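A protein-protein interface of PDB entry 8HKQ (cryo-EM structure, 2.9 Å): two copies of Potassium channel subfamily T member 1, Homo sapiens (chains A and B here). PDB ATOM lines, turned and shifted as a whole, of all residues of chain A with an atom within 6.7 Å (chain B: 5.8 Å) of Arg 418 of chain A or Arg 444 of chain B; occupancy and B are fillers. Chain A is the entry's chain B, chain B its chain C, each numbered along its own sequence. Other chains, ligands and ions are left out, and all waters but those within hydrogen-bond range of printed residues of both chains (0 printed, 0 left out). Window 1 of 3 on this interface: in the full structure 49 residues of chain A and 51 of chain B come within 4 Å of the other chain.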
ATOM      1  N   ASP A 413     -11.041  23.113  25.802  1.00  0.00           N
ATOM      2  CA  ASP A 413     -11.012  21.667  25.950  1.00  0.00           C
ATOM      3  C   ASP A 413     -10.058  21.050  24.928  1.00  0.00           C
ATOM      4  O   ASP A 413      -9.758  21.636  23.884  1.00  0.00           O
ATOM      5  CB  ASP A 413     -12.421  21.092  25.795  1.00  0.00           C
ATOM      6  CG  ASP A 413     -12.465  19.587  25.965  1.00  0.00           C
ATOM      7  OD1 ASP A 413     -11.798  19.072  26.886  1.00  0.00           O
ATOM      8  OD2 ASP A 413     -13.169  18.921  25.176  1.00  0.00           O
ATOM      9  N   VAL A 414      -9.575  19.845  25.247  1.00  0.00           N
ATOM     10  CA  VAL A 414      -8.554  19.204  24.422  1.00  0.00           C
ATOM     11  C   VAL A 414      -9.075  18.935  23.014  1.00  0.00           C
ATOM     12  O   VAL A 414      -8.365  19.160  22.027  1.00  0.00           O
ATOM     13  CB  VAL A 414      -8.043  17.919  25.101  1.00  0.00           C
ATOM     14  CG1 VAL A 414      -7.214  18.266  26.327  1.00  0.00           C
ATOM     15  CG2 VAL A 414      -9.201  17.015  25.491  1.00  0.00           C
ATOM     16  N   GLN A 415     -10.311  18.447  22.894  1.00  0.00           N
ATOM     17  CA  GLN A 415     -10.882  18.207  21.571  1.00  0.00           C
ATOM     18  C   GLN A 415     -11.058  19.513  20.804  1.00  0.00           C
ATOM     19  O   GLN A 415     -10.833  19.564  19.585  1.00  0.00           O
ATOM     20  CB  GLN A 415     -12.215  17.473  21.706  1.00  0.00           C
ATOM     21  CG  GLN A 415     -12.156  16.267  22.628  1.00  0.00           C
ATOM     22  CD  GLN A 415     -13.522  15.846  23.127  1.00  0.00           C
ATOM     23  OE1 GLN A 415     -14.411  15.522  22.340  1.00  0.00           O
ATOM     24  NE2 GLN A 415     -13.697  15.846  24.444  1.00  0.00           N
ATOM     25  N   VAL A 416     -11.458  20.577  21.502  1.00  0.00           N
ATOM     26  CA  VAL A 416     -11.541  21.889  20.870  1.00  0.00           C
ATOM     27  C   VAL A 416     -10.168  22.324  20.377  1.00  0.00           C
ATOM     28  O   VAL A 416     -10.037  22.900  19.294  1.00  0.00           O
ATOM     29  CB  VAL A 416     -12.153  22.916  21.842  1.00  0.00           C
ATOM     30  CG1 VAL A 416     -12.388  24.241  21.134  1.00  0.00           C
ATOM     31  CG2 VAL A 416     -13.449  22.381  22.427  1.00  0.00           C
ATOM     32  N   ARG A 417      -9.121  22.051  21.157  1.00  0.00           N
ATOM     33  CA  ARG A 417      -7.769  22.370  20.709  1.00  0.00           C
ATOM     34  C   ARG A 417      -7.404  21.580  19.456  1.00  0.00           C
ATOM     35  O   ARG A 417      -6.849  22.129  18.497  1.00  0.00           O
ATOM     36  CB  ARG A 417      -6.771  22.095  21.833  1.00  0.00           C
ATOM     37  CG  ARG A 417      -6.313  23.340  22.563  1.00  0.00           C
ATOM     38  CD  ARG A 417      -5.078  23.071  23.399  1.00  0.00           C
ATOM     39  NE  ARG A 417      -4.569  24.298  23.997  1.00  0.00           N
ATOM     40  CZ  ARG A 417      -4.972  24.781  25.164  1.00  0.00           C
ATOM     41  NH1 ARG A 417      -5.889  24.161  25.888  1.00  0.00           N
ATOM     42  NH2 ARG A 417      -4.445  25.915  25.614  1.00  0.00           N
ATOM     43  N   ARG A 418      -7.726  20.285  19.442  1.00  0.00           N
ATOM     44  CA  ARG A 418      -7.404  19.457  18.284  1.00  0.00           C
ATOM     45  C   ARG A 418      -8.102  19.963  17.030  1.00  0.00           C
ATOM     46  O   ARG A 418      -7.516  19.961  15.941  1.00  0.00           O
ATOM     47  CB  ARG A 418      -7.773  17.998  18.560  1.00  0.00           C
ATOM     48  CG  ARG A 418      -6.926  17.343  19.639  1.00  0.00           C
ATOM     49  CD  ARG A 418      -7.301  15.880  19.840  1.00  0.00           C
ATOM     50  NE  ARG A 418      -6.558  15.231  20.918  1.00  0.00           N
ATOM     51  CZ  ARG A 418      -6.776  14.001  21.366  1.00  0.00           C
ATOM     52  NH1 ARG A 418      -7.758  13.250  20.895  1.00  0.00           N
ATOM     53  NH2 ARG A 418      -5.999  13.517  22.332  1.00  0.00           N
ATOM     54  N   VAL A 419      -9.358  20.395  17.157  1.00  0.00           N
ATOM     55  CA  VAL A 419     -10.047  20.897  15.970  1.00  0.00           C
ATOM     56  C   VAL A 419      -9.555  22.294  15.591  1.00  0.00           C
ATOM     57  O   VAL A 419      -9.532  22.645  14.405  1.00  0.00           O
ATOM     58  CB  VAL A 419     -11.577  20.858  16.159  1.00  0.00           C
ATOM     59  CG1 VAL A 419     -12.024  21.800  17.254  1.00  0.00           C
ATOM     60  CG2 VAL A 419     -12.280  21.187  14.849  1.00  0.00           C
ATOM     61  N   LEU A 420      -9.137  23.109  16.566  1.00  0.00           N
ATOM     62  CA  LEU A 420      -8.754  24.485  16.266  1.00  0.00           C
ATOM     63  C   LEU A 420      -7.331  24.626  15.741  1.00  0.00           C
ATOM     64  O   LEU A 420      -7.036  25.628  15.082  1.00  0.00           O
ATOM     65  CB  LEU A 420      -8.926  25.372  17.502  1.00  0.00           C
ATOM     66  CG  LEU A 420     -10.364  25.664  17.936  1.00  0.00           C
ATOM     67  CD1 LEU A 420     -10.430  26.959  18.732  1.00  0.00           C
ATOM     68  CD2 LEU A 420     -11.303  25.705  16.737  1.00  0.00           C
ATOM     69  N   GLN A 421      -6.444  23.670  16.013  1.00  0.00           N
ATOM     70  CA  GLN A 421      -5.145  23.629  15.353  1.00  0.00           C
ATOM     71  C   GLN A 421      -5.173  22.899  14.018  1.00  0.00           C
ATOM     72  O   GLN A 421      -4.111  22.689  13.422  1.00  0.00           O
ATOM     73  CB  GLN A 421      -4.083  23.014  16.275  1.00  0.00           C
ATOM     74  CG  GLN A 421      -3.485  23.952  17.343  1.00  0.00           C
ATOM     75  CD  GLN A 421      -4.470  24.553  18.333  1.00  0.00           C
ATOM     76  OE1 GLN A 421      -5.679  24.370  18.235  1.00  0.00           O
ATOM     77  NE2 GLN A 421      -3.941  25.289  19.301  1.00  0.00           N
ATOM     78  N   ILE A 422      -6.346  22.498  13.542  1.00  0.00           N
ATOM     79  CA  ILE A 422      -6.457  22.105  12.134  1.00  0.00           C
ATOM     80  C   ILE A 422      -6.215  23.334  11.264  1.00  0.00           C
ATOM     81  O   ILE A 422      -6.716  24.429  11.590  1.00  0.00           O
ATOM     82  CB  ILE A 422      -7.838  21.486  11.854  1.00  0.00           C
ATOM     83  CG1 ILE A 422      -7.844  20.007  12.246  1.00  0.00           C
ATOM     84  CG2 ILE A 422      -8.233  21.651  10.395  1.00  0.00           C
ATOM     85  CD1 ILE A 422      -9.134  19.293  11.916  1.00  0.00           C
ATOM     86  N   LYS B 358      -0.570  19.027  23.645  1.00  0.00           N
ATOM     87  CA  LYS B 358      -1.835  19.044  24.367  1.00  0.00           C
ATOM     88  C   LYS B 358      -3.010  19.218  23.411  1.00  0.00           C
ATOM     89  O   LYS B 358      -3.324  18.323  22.626  1.00  0.00           O
ATOM     90  CB  LYS B 358      -1.839  20.158  25.416  1.00  0.00           C
ATOM     91  CG  LYS B 358      -1.372  21.505  24.891  1.00  0.00           C
ATOM     92  CD  LYS B 358      -1.464  22.576  25.966  1.00  0.00           C
ATOM     93  CE  LYS B 358      -0.951  23.915  25.460  1.00  0.00           C
ATOM     94  NZ  LYS B 358      -1.204  25.012  26.435  1.00  0.00           N
ATOM     95  N   VAL B 405      -4.826  -2.248  21.918  1.00  0.00           N
ATOM     96  CA  VAL B 405      -5.245  -0.853  21.879  1.00  0.00           C
ATOM     97  C   VAL B 405      -6.266  -0.635  22.983  1.00  0.00           C
ATOM     98  O   VAL B 405      -7.233  -1.396  23.110  1.00  0.00           O
ATOM     99  CB  VAL B 405      -5.827  -0.478  20.504  1.00  0.00           C
ATOM    100  CG1 VAL B 405      -5.899   1.032  20.357  1.00  0.00           C
ATOM    101  CG2 VAL B 405      -4.995  -1.088  19.391  1.00  0.00           C
ATOM    102  N   LEU B 432      -5.172   4.968  23.650  1.00  0.00           N
ATOM    103  CA  LEU B 432      -5.862   6.050  22.963  1.00  0.00           C
ATOM    104  C   LEU B 432      -6.890   6.664  23.902  1.00  0.00           C
ATOM    105  O   LEU B 432      -7.719   5.948  24.473  1.00  0.00           O
ATOM    106  CB  LEU B 432      -6.548   5.547  21.692  1.00  0.00           C
ATOM    107  CG  LEU B 432      -5.676   4.833  20.659  1.00  0.00           C
ATOM    108  CD1 LEU B 432      -6.434   4.676  19.353  1.00  0.00           C
ATOM    109  CD2 LEU B 432      -4.375   5.588  20.437  1.00  0.00           C
ATOM    110  N   GLN B 433      -6.833   7.982  24.061  1.00  0.00           N
ATOM    111  CA  GLN B 433      -7.795   8.701  24.887  1.00  0.00           C
ATOM    112  C   GLN B 433      -8.984   9.077  24.009  1.00  0.00           C
ATOM    113  O   GLN B 433      -8.910  10.024  23.220  1.00  0.00           O
ATOM    114  CB  GLN B 433      -7.159   9.932  25.523  1.00  0.00           C
ATOM    115  CG  GLN B 433      -8.150  10.866  26.196  1.00  0.00           C
ATOM    116  CD  GLN B 433      -7.482  11.838  27.146  1.00  0.00           C
ATOM    117  OE1 GLN B 433      -6.271  11.783  27.358  1.00  0.00           O
ATOM    118  NE2 GLN B 433      -8.270  12.735  27.726  1.00  0.00           N
ATOM    119  N   GLY B 434     -10.072   8.330  24.142  1.00  0.00           N
ATOM    120  CA  GLY B 434     -11.241   8.580  23.327  1.00  0.00           C
ATOM    121  C   GLY B 434     -12.414   7.754  23.801  1.00  0.00           C
ATOM    122  O   GLY B 434     -12.338   7.048  24.808  1.00  0.00           O
ATOM    123  N   ASP B 439     -16.959   7.814  16.162  1.00  0.00           N
ATOM    124  CA  ASP B 439     -16.378   6.954  15.139  1.00  0.00           C
ATOM    125  C   ASP B 439     -14.916   7.279  14.867  1.00  0.00           C
ATOM    126  O   ASP B 439     -14.165   6.388  14.454  1.00  0.00           O
ATOM    127  CB  ASP B 439     -17.184   7.056  13.845  1.00  0.00           C
ATOM    128  CG  ASP B 439     -18.649   6.723  14.044  1.00  0.00           C
ATOM    129  OD1 ASP B 439     -19.418   7.626  14.435  1.00  0.00           O
ATOM    130  OD2 ASP B 439     -19.032   5.558  13.808  1.00  0.00           O
ATOM    131  N   GLN B 440     -14.498   8.528  15.084  1.00  0.00           N
ATOM    132  CA  GLN B 440     -13.102   8.896  14.863  1.00  0.00           C
ATOM    133  C   GLN B 440     -12.179   8.124  15.798  1.00  0.00           C
ATOM    134  O   GLN B 440     -11.150   7.585  15.373  1.00  0.00           O
ATOM    135  CB  GLN B 440     -12.926  10.401  15.051  1.00  0.00           C
ATOM    136  CG  GLN B 440     -14.114  11.226  14.584  1.00  0.00           C
ATOM    137  CD  GLN B 440     -15.058  11.582  15.716  1.00  0.00           C
ATOM    138  OE1 GLN B 440     -14.639  11.742  16.862  1.00  0.00           O
ATOM    139  NE2 GLN B 440     -16.341  11.707  15.399  1.00  0.00           N
ATOM    140  N   ASP B 441     -12.542   8.051  17.082  1.00  0.00           N
ATOM    141  CA  ASP B 441     -11.763   7.256  18.024  1.00  0.00           C
ATOM    142  C   ASP B 441     -11.815   5.778  17.673  1.00  0.00           C
ATOM    143  O   ASP B 441     -10.906   5.022  18.035  1.00  0.00           O
ATOM    144  CB  ASP B 441     -12.269   7.480  19.446  1.00  0.00           C
ATOM    145  CG  ASP B 441     -12.400   8.947  19.792  1.00  0.00           C
ATOM    146  OD1 ASP B 441     -11.662   9.765  19.207  1.00  0.00           O
ATOM    147  OD2 ASP B 441     -13.243   9.281  20.650  1.00  0.00           O
ATOM    148  N   LEU B 442     -12.867   5.348  16.977  1.00  0.00           N
ATOM    149  CA  LEU B 442     -12.972   3.955  16.571  1.00  0.00           C
ATOM    150  C   LEU B 442     -12.053   3.627  15.402  1.00  0.00           C
ATOM    151  O   LEU B 442     -11.469   2.539  15.369  1.00  0.00           O
ATOM    152  CB  LEU B 442     -14.422   3.622  16.219  1.00  0.00           C
ATOM    153  CG  LEU B 442     -15.361   3.525  17.425  1.00  0.00           C
ATOM    154  CD1 LEU B 442     -16.670   2.868  17.046  1.00  0.00           C
ATOM    155  CD2 LEU B 442     -14.703   2.782  18.566  1.00  0.00           C
ATOM    156  N   MET B 443     -11.904   4.541  14.439  1.00  0.00           N
ATOM    157  CA  MET B 443     -10.965   4.295  13.350  1.00  0.00           C
ATOM    158  C   MET B 443      -9.523   4.546  13.761  1.00  0.00           C
ATOM    159  O   MET B 443      -8.609   3.968  13.162  1.00  0.00           O
ATOM    160  CB  MET B 443     -11.297   5.149  12.122  1.00  0.00           C
ATOM    161  CG  MET B 443     -11.918   6.491  12.416  1.00  0.00           C
ATOM    162  SD  MET B 443     -12.147   7.474  10.922  1.00  0.00           S
ATOM    163  CE  MET B 443     -13.607   6.701  10.230  1.00  0.00           C
ATOM    164  N   ARG B 444      -9.294   5.400  14.763  1.00  0.00           N
ATOM    165  CA  ARG B 444      -7.950   5.519  15.317  1.00  0.00           C
ATOM    166  C   ARG B 444      -7.497   4.208  15.944  1.00  0.00           C
ATOM    167  O   ARG B 444      -6.319   3.846  15.847  1.00  0.00           O
ATOM    168  CB  ARG B 444      -7.891   6.648  16.345  1.00  0.00           C
ATOM    169  CG  ARG B 444      -8.054   8.037  15.757  1.00  0.00           C
ATOM    170  CD  ARG B 444      -8.279   9.067  16.850  1.00  0.00           C
ATOM    171  NE  ARG B 444      -7.350   8.886  17.958  1.00  0.00           N
ATOM    172  CZ  ARG B 444      -7.492   9.442  19.153  1.00  0.00           C
ATOM    173  NH1 ARG B 444      -8.524  10.221  19.436  1.00  0.00           N
ATOM    174  NH2 ARG B 444      -6.577   9.209  20.089  1.00  0.00           N
ATOM    175  N   ALA B 445      -8.413   3.488  16.591  1.00  0.00           N
ATOM    176  CA  ALA B 445      -8.111   2.172  17.135  1.00  0.00           C
ATOM    177  C   ALA B 445      -8.217   1.064  16.097  1.00  0.00           C
ATOM    178  O   ALA B 445      -7.886  -0.085  16.411  1.00  0.00           O
ATOM    179  CB  ALA B 445      -9.041   1.866  18.312  1.00  0.00           C
ATOM    180  N   LYS B 446      -8.669   1.380  14.882  1.00  0.00           N
ATOM    181  CA  LYS B 446      -8.769   0.421  13.782  1.00  0.00           C
ATOM    182  C   LYS B 446      -9.652  -0.768  14.164  1.00  0.00           C
ATOM    183  O   LYS B 446      -9.249  -1.931  14.102  1.00  0.00           O
ATOM    184  CB  LYS B 446      -7.376  -0.035  13.332  1.00  0.00           C
ATOM    185  CG  LYS B 446      -6.471   1.106  12.897  1.00  0.00           C
ATOM    186  CD  LYS B 446      -5.027   0.849  13.286  1.00  0.00           C
ATOM    187  CE  LYS B 446      -4.124   1.982  12.826  1.00  0.00           C
ATOM    188  NZ  LYS B 446      -4.220   2.211  11.359  1.00  0.00           N
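Arg 418 of chain A touches just one residue of chain B: Arg 444 (3.4 Å). Of chain A, only Arg 418 comes within 4 Å of Arg 444 of chain B. Printed residues of chain A within 4 Å of Lys 358 of chain B: Arg 417. Of the printed residues of chain B, Arg 417 of chain A touches Lys 358 (3.5 Å). Val 419 of chain A touches none of the printed residues of chain B. Asp 439 of chain B touches none of the printed residues of chain A. The nearest printed residue of chain A that does not touch Arg 444 of chain B is Gln 415 of chain A (7.7 Å).
No position is printed for both chains.
NZ of Lys 358 of chain B lies close to NH2 of Arg 417 of chain A, 3.5 Å away. The guanidinium group of Arg 418 of chain A sits close to the guanidinium group of Arg 444 of chain B.
NH1 of Arg 444 of chain B is in salt-bridge range of OD1 of Asp 441 of chain B (3.2 Å). O of Arg 417 of chain A sits close to OE1 of Gln 421 of chain A (2.5 Å).
Of the 13 printed residues of chain B, 2 touch a printed residue of chain A. Among the printed residues, 2 pairs touch across the chains. Among the printed residues, no Asp or Glu carboxylate lies within 4 Å of a Lys or Arg side-chain nitrogen of the other chain.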
